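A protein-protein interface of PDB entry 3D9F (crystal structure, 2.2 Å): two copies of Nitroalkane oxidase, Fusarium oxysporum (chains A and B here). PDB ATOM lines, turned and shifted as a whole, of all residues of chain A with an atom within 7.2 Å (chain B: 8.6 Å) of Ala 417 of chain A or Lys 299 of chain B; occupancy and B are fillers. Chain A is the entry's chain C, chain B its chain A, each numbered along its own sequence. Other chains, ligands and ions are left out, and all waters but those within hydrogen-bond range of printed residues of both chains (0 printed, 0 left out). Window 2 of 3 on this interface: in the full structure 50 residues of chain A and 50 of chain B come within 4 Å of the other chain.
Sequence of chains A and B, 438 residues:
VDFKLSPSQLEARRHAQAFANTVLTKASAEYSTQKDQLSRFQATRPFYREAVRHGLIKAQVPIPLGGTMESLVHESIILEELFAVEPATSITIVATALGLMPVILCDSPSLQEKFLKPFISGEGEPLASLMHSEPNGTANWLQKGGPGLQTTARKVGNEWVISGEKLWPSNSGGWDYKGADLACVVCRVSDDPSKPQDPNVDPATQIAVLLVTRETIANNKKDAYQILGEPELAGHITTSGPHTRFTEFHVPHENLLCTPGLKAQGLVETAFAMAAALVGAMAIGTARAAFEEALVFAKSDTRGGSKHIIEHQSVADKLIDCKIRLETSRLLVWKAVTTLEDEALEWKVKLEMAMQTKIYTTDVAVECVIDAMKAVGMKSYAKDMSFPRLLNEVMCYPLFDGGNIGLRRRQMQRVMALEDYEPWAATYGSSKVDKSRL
NZ of Lys 299 of chain B is in hydrogen-bond range of O of Ala 417 of chain A (3.4 Å).
O of Ile 310 of chain B lies within hydrogen-bond range of NE2 of Gln 413 of chain A (3.1 Å).
The backbone carbonyl oxygen (O) of Glu 311 of chain B sits at hydrogen-bond distance from the side-chain amide nitrogen (NE2) of Gln 413 of chain A (3.2 Å).
The side-chain amino group (NZ) of Lys 299 of chain B is in hydrogen-bond range of the backbone carbonyl oxygen (O) of Leu 418 of chain A (2.7 Å).
The backbone carbonyl oxygen (O) of Met 416 of chain A sits at hydrogen-bond distance from the side-chain amino group (NZ) of Lys 299 of chain B (2.8 Å).
Among the printed residues, pairs that only touch across the chains: Gln 413 of chain A with His 312 of chain B (3.9 Å), Gln 413 of chain A with Ala 316 of chain B (3.3 Å), Met 416 of chain A with Ile 310 of chain B (3.6 Å), Met 416 of chain A with Leu 319 of chain B (3.9 Å), Ala 417 of chain A with Ile 310 of chain B (3.6 Å), Ala 417 of chain A with Glu 311 of chain B (3.3 Å) and Tyr 421 of chain A with Leu 295 of chain B (3.9 Å).
No position is printed for both chains.
Of the 12 pairs that touch across the chains among the printed residues, none has its exchanged pair printed and touching as well.
O of Ala 298 of chain B is in hydrogen-bond range of N of Ile 310 of chain B.
The backbone carbonyl oxygen (O) of Lys 299 of chain B sits close to a ring nitrogen (NE2) of His 308 of chain B, at 3.3 Å.
Of the 11 printed residues of chain A, 5 touch a printed residue of chain B.
Printed residues of chain A that touch a printed residue of chain B: Gln 413, Met 416, Ala 417, Leu 418 and Tyr 421.
Lys 299 of chain B touches just these residues of chain A: Met 416 (2.8 Å), Ala 417 (3.4 Å) and Leu 418 (2.7 Å).
Of the printed residues of chain A, Glu 311 of chain B touches Gln 413 and Ala 417.
Of the printed residues of chain A, Leu 319 of chain B touches Met 416.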
ATOM      1  N   MET A 412      13.907  -3.447  16.338  1.00  0.00           N
ATOM      2  CA  MET A 412      13.106  -2.956  17.448  1.00  0.00           C
ATOM      3  C   MET A 412      11.792  -3.735  17.606  1.00  0.00           C
ATOM      4  O   MET A 412      11.437  -4.154  18.716  1.00  0.00           O
ATOM      5  CB  MET A 412      12.820  -1.465  17.315  1.00  0.00           C
ATOM      6  CG  MET A 412      12.065  -0.930  18.536  1.00  0.00           C
ATOM      7  SD  MET A 412      11.927   0.849  18.563  1.00  0.00           S
ATOM      8  CE  MET A 412      10.906   1.056  20.020  1.00  0.00           C
ATOM      9  N   GLN A 413      11.069  -3.902  16.498  1.00  0.00           N
ATOM     10  CA  GLN A 413       9.831  -4.669  16.451  1.00  0.00           C
ATOM     11  C   GLN A 413      10.005  -6.047  17.088  1.00  0.00           C
ATOM     12  O   GLN A 413       9.152  -6.487  17.846  1.00  0.00           O
ATOM     13  CB  GLN A 413       9.378  -4.824  14.989  1.00  0.00           C
ATOM     14  CG  GLN A 413       8.179  -5.779  14.737  1.00  0.00           C
ATOM     15  CD  GLN A 413       7.803  -5.877  13.250  1.00  0.00           C
ATOM     16  OE1 GLN A 413       8.496  -5.337  12.371  1.00  0.00           O
ATOM     17  NE2 GLN A 413       6.690  -6.553  12.973  1.00  0.00           N
ATOM     18  N   ARG A 414      11.085  -6.733  16.730  1.00  0.00           N
ATOM     19  CA  ARG A 414      11.367  -8.067  17.233  1.00  0.00           C
ATOM     20  C   ARG A 414      11.454  -8.090  18.777  1.00  0.00           C
ATOM     21  O   ARG A 414      10.891  -8.960  19.426  1.00  0.00           O
ATOM     22  CB  ARG A 414      12.671  -8.620  16.580  1.00  0.00           C
ATOM     23  N   VAL A 415      12.145  -7.113  19.353  1.00  0.00           N
ATOM     24  CA  VAL A 415      12.220  -6.949  20.813  1.00  0.00           C
ATOM     25  C   VAL A 415      10.835  -6.732  21.459  1.00  0.00           C
ATOM     26  O   VAL A 415      10.523  -7.325  22.502  1.00  0.00           O
ATOM     27  CB  VAL A 415      13.183  -5.787  21.200  1.00  0.00           C
ATOM     28  CG1 VAL A 415      13.108  -5.494  22.689  1.00  0.00           C
ATOM     29  CG2 VAL A 415      14.617  -6.141  20.807  1.00  0.00           C
ATOM     30  N   MET A 416      10.012  -5.894  20.839  1.00  0.00           N
ATOM     31  CA  MET A 416       8.726  -5.495  21.419  1.00  0.00           C
ATOM     32  C   MET A 416       7.714  -6.634  21.388  1.00  0.00           C
ATOM     33  O   MET A 416       6.788  -6.666  22.193  1.00  0.00           O
ATOM     34  CB  MET A 416       8.133  -4.279  20.685  1.00  0.00           C
ATOM     35  CG  MET A 416       8.936  -3.002  20.770  1.00  0.00           C
ATOM     36  SD  MET A 416       8.251  -1.700  19.682  1.00  0.00           S
ATOM     37  CE  MET A 416       6.834  -1.204  20.680  1.00  0.00           C
ATOM     38  N   ALA A 417       7.903  -7.550  20.443  1.00  0.00           N
ATOM     39  CA  ALA A 417       7.030  -8.697  20.264  1.00  0.00           C
ATOM     40  C   ALA A 417       7.345  -9.837  21.250  1.00  0.00           C
ATOM     41  O   ALA A 417       6.499 -10.698  21.479  1.00  0.00           O
ATOM     42  CB  ALA A 417       7.106  -9.198  18.829  1.00  0.00           C
ATOM     43  N   LEU A 418       8.555  -9.843  21.820  1.00  0.00           N
ATOM     44  CA  LEU A 418       8.928 -10.850  22.820  1.00  0.00           C
ATOM     45  C   LEU A 418       7.980 -10.792  24.019  1.00  0.00           C
ATOM     46  O   LEU A 418       7.526  -9.707  24.418  1.00  0.00           O
ATOM     47  CB  LEU A 418      10.372 -10.671  23.273  1.00  0.00           C
ATOM     48  CG  LEU A 418      11.448 -10.860  22.200  1.00  0.00           C
ATOM     49  CD1 LEU A 418      12.808 -10.464  22.732  1.00  0.00           C
ATOM     50  CD2 LEU A 418      11.492 -12.281  21.645  1.00  0.00           C
ATOM     51  N   GLU A 419       7.680 -11.958  24.591  1.00  0.00           N
ATOM     52  CA  GLU A 419       6.738 -12.038  25.718  1.00  0.00           C
ATOM     53  C   GLU A 419       7.202 -11.303  26.980  1.00  0.00           C
ATOM     54  O   GLU A 419       6.373 -10.782  27.733  1.00  0.00           O
ATOM     55  CB  GLU A 419       6.402 -13.489  26.045  1.00  0.00           C
ATOM     56  CG  GLU A 419       5.511 -14.145  24.982  1.00  0.00           C
ATOM     57  CD  GLU A 419       4.580 -15.225  25.554  1.00  0.00           C
ATOM     58  OE1 GLU A 419       5.066 -16.113  26.302  1.00  0.00           O
ATOM     59  OE2 GLU A 419       3.361 -15.187  25.244  1.00  0.00           O
ATOM     60  N   ASP A 420       8.514 -11.260  27.197  1.00  0.00           N
ATOM     61  CA  ASP A 420       9.080 -10.614  28.376  1.00  0.00           C
ATOM     62  C   ASP A 420       9.469  -9.134  28.185  1.00  0.00           C
ATOM     63  O   ASP A 420       9.993  -8.501  29.108  1.00  0.00           O
ATOM     64  CB  ASP A 420      10.271 -11.427  28.918  1.00  0.00           C
ATOM     65  CG  ASP A 420      11.252 -11.836  27.826  1.00  0.00           C
ATOM     66  OD1 ASP A 420      10.819 -12.082  26.673  1.00  0.00           O
ATOM     67  OD2 ASP A 420      12.460 -11.939  28.121  1.00  0.00           O
ATOM     68  N   TYR A 421       9.193  -8.585  27.004  1.00  0.00           N
ATOM     69  CA  TYR A 421       9.353  -7.152  26.736  1.00  0.00           C
ATOM     70  C   TYR A 421       8.866  -6.250  27.864  1.00  0.00           C
ATOM     71  O   TYR A 421       7.701  -6.256  28.216  1.00  0.00           O
ATOM     72  CB  TYR A 421       8.625  -6.763  25.445  1.00  0.00           C
ATOM     73  CG  TYR A 421       8.719  -5.290  25.079  1.00  0.00           C
ATOM     74  CD1 TYR A 421       7.561  -4.526  24.902  1.00  0.00           C
ATOM     75  CD2 TYR A 421       9.971  -4.665  24.898  1.00  0.00           C
ATOM     76  CE1 TYR A 421       7.634  -3.182  24.543  1.00  0.00           C
ATOM     77  CE2 TYR A 421      10.058  -3.319  24.540  1.00  0.00           C
ATOM     78  CZ  TYR A 421       8.884  -2.588  24.359  1.00  0.00           C
ATOM     79  OH  TYR A 421       8.948  -1.270  24.006  1.00  0.00           O
ATOM     80  N   GLU A 422       9.779  -5.451  28.400  1.00  0.00           N
ATOM     81  CA  GLU A 422       9.452  -4.466  29.411  1.00  0.00           C
ATOM     82  C   GLU A 422       9.750  -3.086  28.841  1.00  0.00           C
ATOM     83  O   GLU A 422      10.911  -2.672  28.839  1.00  0.00           O
ATOM     84  CB  GLU A 422      10.314  -4.716  30.659  1.00  0.00           C
ATOM     85  CG  GLU A 422       9.711  -5.655  31.702  1.00  0.00           C
ATOM     86  CD  GLU A 422      10.448  -5.563  33.049  1.00  0.00           C
ATOM     87  OE1 GLU A 422       9.859  -5.004  34.016  1.00  0.00           O
ATOM     88  OE2 GLU A 422      11.618  -6.014  33.130  1.00  0.00           O
ATOM     89  N   PHE B 291      -0.787   3.798  24.560  1.00  0.00           N
ATOM     90  CA  PHE B 291       0.240   2.945  23.979  1.00  0.00           C
ATOM     91  C   PHE B 291       0.258   1.541  24.598  1.00  0.00           C
ATOM     92  O   PHE B 291       0.462   0.551  23.877  1.00  0.00           O
ATOM     93  CB  PHE B 291       1.606   3.625  24.062  1.00  0.00           C
ATOM     94  CG  PHE B 291       2.775   2.678  23.973  1.00  0.00           C
ATOM     95  CD1 PHE B 291       3.241   2.242  22.742  1.00  0.00           C
ATOM     96  CD2 PHE B 291       3.424   2.238  25.127  1.00  0.00           C
ATOM     97  CE1 PHE B 291       4.332   1.385  22.643  1.00  0.00           C
ATOM     98  CE2 PHE B 291       4.516   1.379  25.045  1.00  0.00           C
ATOM     99  CZ  PHE B 291       4.969   0.940  23.798  1.00  0.00           C
ATOM    100  N   GLU B 292       0.070   1.458  25.920  1.00  0.00           N
ATOM    101  CA  GLU B 292       0.110   0.178  26.635  1.00  0.00           C
ATOM    102  C   GLU B 292      -1.132  -0.653  26.307  1.00  0.00           C
ATOM    103  O   GLU B 292      -1.016  -1.851  26.035  1.00  0.00           O
ATOM    104  CB  GLU B 292       0.275   0.359  28.151  1.00  0.00           C
ATOM    105  CG  GLU B 292       1.745   0.533  28.575  1.00  0.00           C
ATOM    106  CD  GLU B 292       1.958   1.013  30.019  1.00  0.00           C
ATOM    107  OE1 GLU B 292       1.030   0.946  30.869  1.00  0.00           O
ATOM    108  OE2 GLU B 292       3.083   1.468  30.300  1.00  0.00           O
ATOM    109  N   GLU B 293      -2.301  -0.022  26.299  1.00  0.00           N
ATOM    110  CA  GLU B 293      -3.502  -0.723  25.856  1.00  0.00           C
ATOM    111  C   GLU B 293      -3.304  -1.304  24.443  1.00  0.00           C
ATOM    112  O   GLU B 293      -3.472  -2.496  24.249  1.00  0.00           O
ATOM    113  CB  GLU B 293      -4.743   0.160  25.916  1.00  0.00           C
ATOM    114  CG  GLU B 293      -6.065  -0.662  25.845  1.00  0.00           C
ATOM    115  CD  GLU B 293      -7.248   0.063  26.472  1.00  0.00           C
ATOM    116  OE1 GLU B 293      -7.156   0.461  27.656  1.00  0.00           O
ATOM    117  OE2 GLU B 293      -8.280   0.226  25.794  1.00  0.00           O
ATOM    118  N   ALA B 294      -2.906  -0.473  23.476  1.00  0.00           N
ATOM    119  CA  ALA B 294      -2.649  -0.968  22.119  1.00  0.00           C
ATOM    120  C   ALA B 294      -1.569  -2.046  22.022  1.00  0.00           C
ATOM    121  O   ALA B 294      -1.708  -2.994  21.250  1.00  0.00           O
ATOM    122  CB  ALA B 294      -2.325   0.185  21.182  1.00  0.00           C
ATOM    123  N   LEU B 295      -0.493  -1.900  22.794  1.00  0.00           N
ATOM    124  CA  LEU B 295       0.585  -2.876  22.812  1.00  0.00           C
ATOM    125  C   LEU B 295       0.124  -4.243  23.336  1.00  0.00           C
ATOM    126  O   LEU B 295       0.422  -5.272  22.729  1.00  0.00           O
ATOM    127  CB  LEU B 295       1.752  -2.350  23.654  1.00  0.00           C
ATOM    128  CG  LEU B 295       3.007  -3.180  23.905  1.00  0.00           C
ATOM    129  CD1 LEU B 295       3.883  -3.364  22.645  1.00  0.00           C
ATOM    130  CD2 LEU B 295       3.810  -2.555  25.061  1.00  0.00           C
ATOM    131  N   VAL B 296      -0.575  -4.251  24.469  1.00  0.00           N
ATOM    132  CA  VAL B 296      -1.089  -5.499  25.050  1.00  0.00           C
ATOM    133  C   VAL B 296      -2.025  -6.217  24.039  1.00  0.00           C
ATOM    134  O   VAL B 296      -1.851  -7.407  23.734  1.00  0.00           O
ATOM    135  CB  VAL B 296      -1.728  -5.237  26.443  1.00  0.00           C
ATOM    136  CG1 VAL B 296      -2.606  -6.421  26.903  1.00  0.00           C
ATOM    137  CG2 VAL B 296      -0.619  -4.956  27.479  1.00  0.00           C
ATOM    138  N   PHE B 297      -2.958  -5.453  23.478  1.00  0.00           N
ATOM    139  CA  PHE B 297      -3.794  -5.903  22.383  1.00  0.00           C
ATOM    140  C   PHE B 297      -3.002  -6.495  21.218  1.00  0.00           C
ATOM    141  O   PHE B 297      -3.328  -7.591  20.738  1.00  0.00           O
ATOM    142  CB  PHE B 297      -4.692  -4.763  21.885  1.00  0.00           C
ATOM    143  CG  PHE B 297      -5.700  -5.197  20.843  1.00  0.00           C
ATOM    144  CD1 PHE B 297      -6.950  -5.708  21.228  1.00  0.00           C
ATOM    145  CD2 PHE B 297      -5.404  -5.116  19.482  1.00  0.00           C
ATOM    146  CE1 PHE B 297      -7.890  -6.110  20.264  1.00  0.00           C
ATOM    147  CE2 PHE B 297      -6.346  -5.537  18.509  1.00  0.00           C
ATOM    148  CZ  PHE B 297      -7.578  -6.021  18.911  1.00  0.00           C
ATOM    149  N   ALA B 298      -1.976  -5.778  20.754  1.00  0.00           N
ATOM    150  CA  ALA B 298      -1.220  -6.204  19.567  1.00  0.00           C
ATOM    151  C   ALA B 298      -0.492  -7.506  19.832  1.00  0.00           C
ATOM    152  O   ALA B 298      -0.175  -8.268  18.915  1.00  0.00           O
ATOM    153  CB  ALA B 298      -0.236  -5.142  19.137  1.00  0.00           C
ATOM    154  N   LYS B 299      -0.199  -7.735  21.101  1.00  0.00           N
ATOM    155  CA  LYS B 299       0.576  -8.890  21.504  1.00  0.00           C
ATOM    156  C   LYS B 299      -0.280 -10.121  21.858  1.00  0.00           C
ATOM    157  O   LYS B 299       0.242 -11.215  22.029  1.00  0.00           O
ATOM    158  CB  LYS B 299       1.510  -8.492  22.643  1.00  0.00           C
ATOM    159  CG  LYS B 299       2.754  -7.781  22.126  1.00  0.00           C
ATOM    160  CD  LYS B 299       3.370  -6.898  23.169  1.00  0.00           C
ATOM    161  CE  LYS B 299       4.094  -7.712  24.238  1.00  0.00           C
ATOM    162  NZ  LYS B 299       5.264  -8.417  23.700  1.00  0.00           N
ATOM    163  N   SER B 300      -1.593  -9.940  21.949  1.00  0.00           N
ATOM    164  CA  SER B 300      -2.464 -11.025  22.382  1.00  0.00           C
ATOM    165  C   SER B 300      -3.636 -11.268  21.424  1.00  0.00           C
ATOM    166  O   SER B 300      -4.549 -12.041  21.732  1.00  0.00           O
ATOM    167  CB  SER B 300      -2.961 -10.747  23.806  1.00  0.00           C
ATOM    168  OG  SER B 300      -3.842  -9.642  23.836  1.00  0.00           O
ATOM    169  N   ASP B 301      -3.611 -10.613  20.265  1.00  0.00           N
ATOM    170  CA  ASP B 301      -4.729 -10.675  19.344  1.00  0.00           C
ATOM    171  C   ASP B 301      -4.309 -10.742  17.867  1.00  0.00           C
ATOM    172  O   ASP B 301      -3.521  -9.917  17.370  1.00  0.00           O
ATOM    173  CB  ASP B 301      -5.671  -9.511  19.601  1.00  0.00           C
ATOM    174  CG  ASP B 301      -7.065  -9.773  19.088  1.00  0.00           C
ATOM    175  OD1 ASP B 301      -7.246  -9.863  17.848  1.00  0.00           O
ATOM    176  OD2 ASP B 301      -7.981  -9.875  19.932  1.00  0.00           O
ATOM    177  N   THR B 302      -4.856 -11.730  17.168  1.00  0.00           N
ATOM    178  CA  THR B 302      -4.432 -12.034  15.813  1.00  0.00           C
ATOM    179  C   THR B 302      -5.351 -11.350  14.799  1.00  0.00           C
ATOM    180  O   THR B 302      -5.090 -11.377  13.596  1.00  0.00           O
ATOM    181  CB  THR B 302      -4.388 -13.583  15.565  1.00  0.00           C
ATOM    182  OG1 THR B 302      -5.722 -14.101  15.492  1.00  0.00           O
ATOM    183  CG2 THR B 302      -3.613 -14.301  16.668  1.00  0.00           C
ATOM    184  N   LYS B 307      -1.217 -14.875  13.090  1.00  0.00           N
ATOM    185  CA  LYS B 307      -0.174 -14.375  14.001  1.00  0.00           C
ATOM    186  C   LYS B 307      -0.616 -13.115  14.751  1.00  0.00           C
ATOM    187  O   LYS B 307      -1.510 -12.402  14.279  1.00  0.00           O
ATOM    188  CB  LYS B 307       1.173 -14.194  13.271  1.00  0.00           C
ATOM    189  CG  LYS B 307       1.173 -13.196  12.107  1.00  0.00           C
ATOM    190  CD  LYS B 307       2.490 -13.204  11.318  1.00  0.00           C
ATOM    191  CE  LYS B 307       2.514 -12.057  10.275  1.00  0.00           C
ATOM    192  NZ  LYS B 307       3.819 -11.848   9.561  1.00  0.00           N
ATOM    193  N   HIS B 308      -0.042 -12.874  15.933  1.00  0.00           N
ATOM    194  CA  HIS B 308      -0.375 -11.673  16.710  1.00  0.00           C
ATOM    195  C   HIS B 308      -0.133 -10.445  15.829  1.00  0.00           C
ATOM    196  O   HIS B 308       0.822 -10.419  15.058  1.00  0.00           O
ATOM    197  CB  HIS B 308       0.462 -11.575  17.987  1.00  0.00           C
ATOM    198  CG  HIS B 308       0.158 -12.634  19.014  1.00  0.00           C
ATOM    199  ND1 HIS B 308      -1.125 -12.934  19.433  1.00  0.00           N
ATOM    200  CD2 HIS B 308       0.981 -13.436  19.732  1.00  0.00           C
ATOM    201  CE1 HIS B 308      -1.080 -13.883  20.354  1.00  0.00           C
ATOM    202  NE2 HIS B 308       0.186 -14.213  20.545  1.00  0.00           N
ATOM    203  N   ILE B 309      -0.995  -9.437  15.917  1.00  0.00           N
ATOM    204  CA  ILE B 309      -0.863  -8.299  14.989  1.00  0.00           C
ATOM    205  C   ILE B 309       0.439  -7.476  15.121  1.00  0.00           C
ATOM    206  O   ILE B 309       0.879  -6.869  14.133  1.00  0.00           O
ATOM    207  CB  ILE B 309      -2.111  -7.412  14.914  1.00  0.00           C
ATOM    208  CG1 ILE B 309      -2.419  -6.746  16.266  1.00  0.00           C
ATOM    209  CG2 ILE B 309      -3.280  -8.239  14.364  1.00  0.00           C
ATOM    210  CD1 ILE B 309      -3.261  -5.472  16.164  1.00  0.00           C
ATOM    211  N   ILE B 310       1.082  -7.518  16.293  1.00  0.00           N
ATOM    212  CA  ILE B 310       2.428  -6.932  16.435  1.00  0.00           C
ATOM    213  C   ILE B 310       3.409  -7.450  15.382  1.00  0.00           C
ATOM    214  O   ILE B 310       4.432  -6.807  15.120  1.00  0.00           O
ATOM    215  CB  ILE B 310       3.037  -7.052  17.899  1.00  0.00           C
ATOM    216  CG1 ILE B 310       4.074  -5.932  18.124  1.00  0.00           C
ATOM    217  CG2 ILE B 310       3.636  -8.472  18.168  1.00  0.00           C
ATOM    218  CD1 ILE B 310       4.503  -5.740  19.526  1.00  0.00           C
ATOM    219  N   GLU B 311       3.107  -8.590  14.749  1.00  0.00           N
ATOM    220  CA  GLU B 311       4.026  -9.117  13.732  1.00  0.00           C
ATOM    221  C   GLU B 311       3.861  -8.437  12.364  1.00  0.00           C
ATOM    222  O   GLU B 311       4.709  -8.588  11.487  1.00  0.00           O
ATOM    223  CB  GLU B 311       3.948 -10.649  13.602  1.00  0.00           C
ATOM    224  CG  GLU B 311       4.508 -11.456  14.799  1.00  0.00           C
ATOM    225  CD  GLU B 311       6.003 -11.195  15.102  1.00  0.00           C
ATOM    226  OE1 GLU B 311       6.347 -11.201  16.309  1.00  0.00           O
ATOM    227  OE2 GLU B 311       6.834 -10.991  14.162  1.00  0.00           O
ATOM    228  N   HIS B 312       2.786  -7.677  12.187  1.00  0.00           N
ATOM    229  CA  HIS B 312       2.619  -6.904  10.962  1.00  0.00           C
ATOM    230  C   HIS B 312       3.423  -5.595  11.023  1.00  0.00           C
ATOM    231  O   HIS B 312       3.223  -4.792  11.934  1.00  0.00           O
ATOM    232  CB  HIS B 312       1.137  -6.630  10.745  1.00  0.00           C
ATOM    233  CG  HIS B 312       0.309  -7.878  10.637  1.00  0.00           C
ATOM    234  ND1 HIS B 312       0.635  -8.917   9.787  1.00  0.00           N
ATOM    235  CD2 HIS B 312      -0.829  -8.254  11.269  1.00  0.00           C
ATOM    236  CE1 HIS B 312      -0.274  -9.873   9.894  1.00  0.00           C
ATOM    237  NE2 HIS B 312      -1.182  -9.489  10.774  1.00  0.00           N
ATOM    238  N   VAL B 315       1.632  -2.231  11.855  1.00  0.00           N
ATOM    239  CA  VAL B 315       1.201  -2.165  13.246  1.00  0.00           C
ATOM    240  C   VAL B 315       2.442  -1.847  14.089  1.00  0.00           C
ATOM    241  O   VAL B 315       2.435  -0.892  14.861  1.00  0.00           O
ATOM    242  CB  VAL B 315       0.535  -3.494  13.721  1.00  0.00           C
ATOM    243  CG1 VAL B 315       0.188  -3.434  15.224  1.00  0.00           C
ATOM    244  CG2 VAL B 315      -0.732  -3.816  12.882  1.00  0.00           C
ATOM    245  N   ALA B 316       3.509  -2.619  13.895  1.00  0.00           N
ATOM    246  CA  ALA B 316       4.744  -2.418  14.625  1.00  0.00           C
ATOM    247  C   ALA B 316       5.192  -0.964  14.513  1.00  0.00           C
ATOM    248  O   ALA B 316       5.481  -0.344  15.535  1.00  0.00           O
ATOM    249  CB  ALA B 316       5.828  -3.361  14.132  1.00  0.00           C
ATOM    250  N   LEU B 319       3.324   1.425  16.854  1.00  0.00           N
ATOM    251  CA  LEU B 319       3.747   1.210  18.247  1.00  0.00           C
ATOM    252  C   LEU B 319       5.159   1.745  18.478  1.00  0.00           C
ATOM    253  O   LEU B 319       5.393   2.432  19.463  1.00  0.00           O
ATOM    254  CB  LEU B 319       3.643  -0.272  18.637  1.00  0.00           C
ATOM    255  CG  LEU B 319       2.218  -0.873  18.619  1.00  0.00           C
ATOM    256  CD1 LEU B 319       2.268  -2.399  18.712  1.00  0.00           C
ATOM    257  CD2 LEU B 319       1.299  -0.292  19.693  1.00  0.00           C
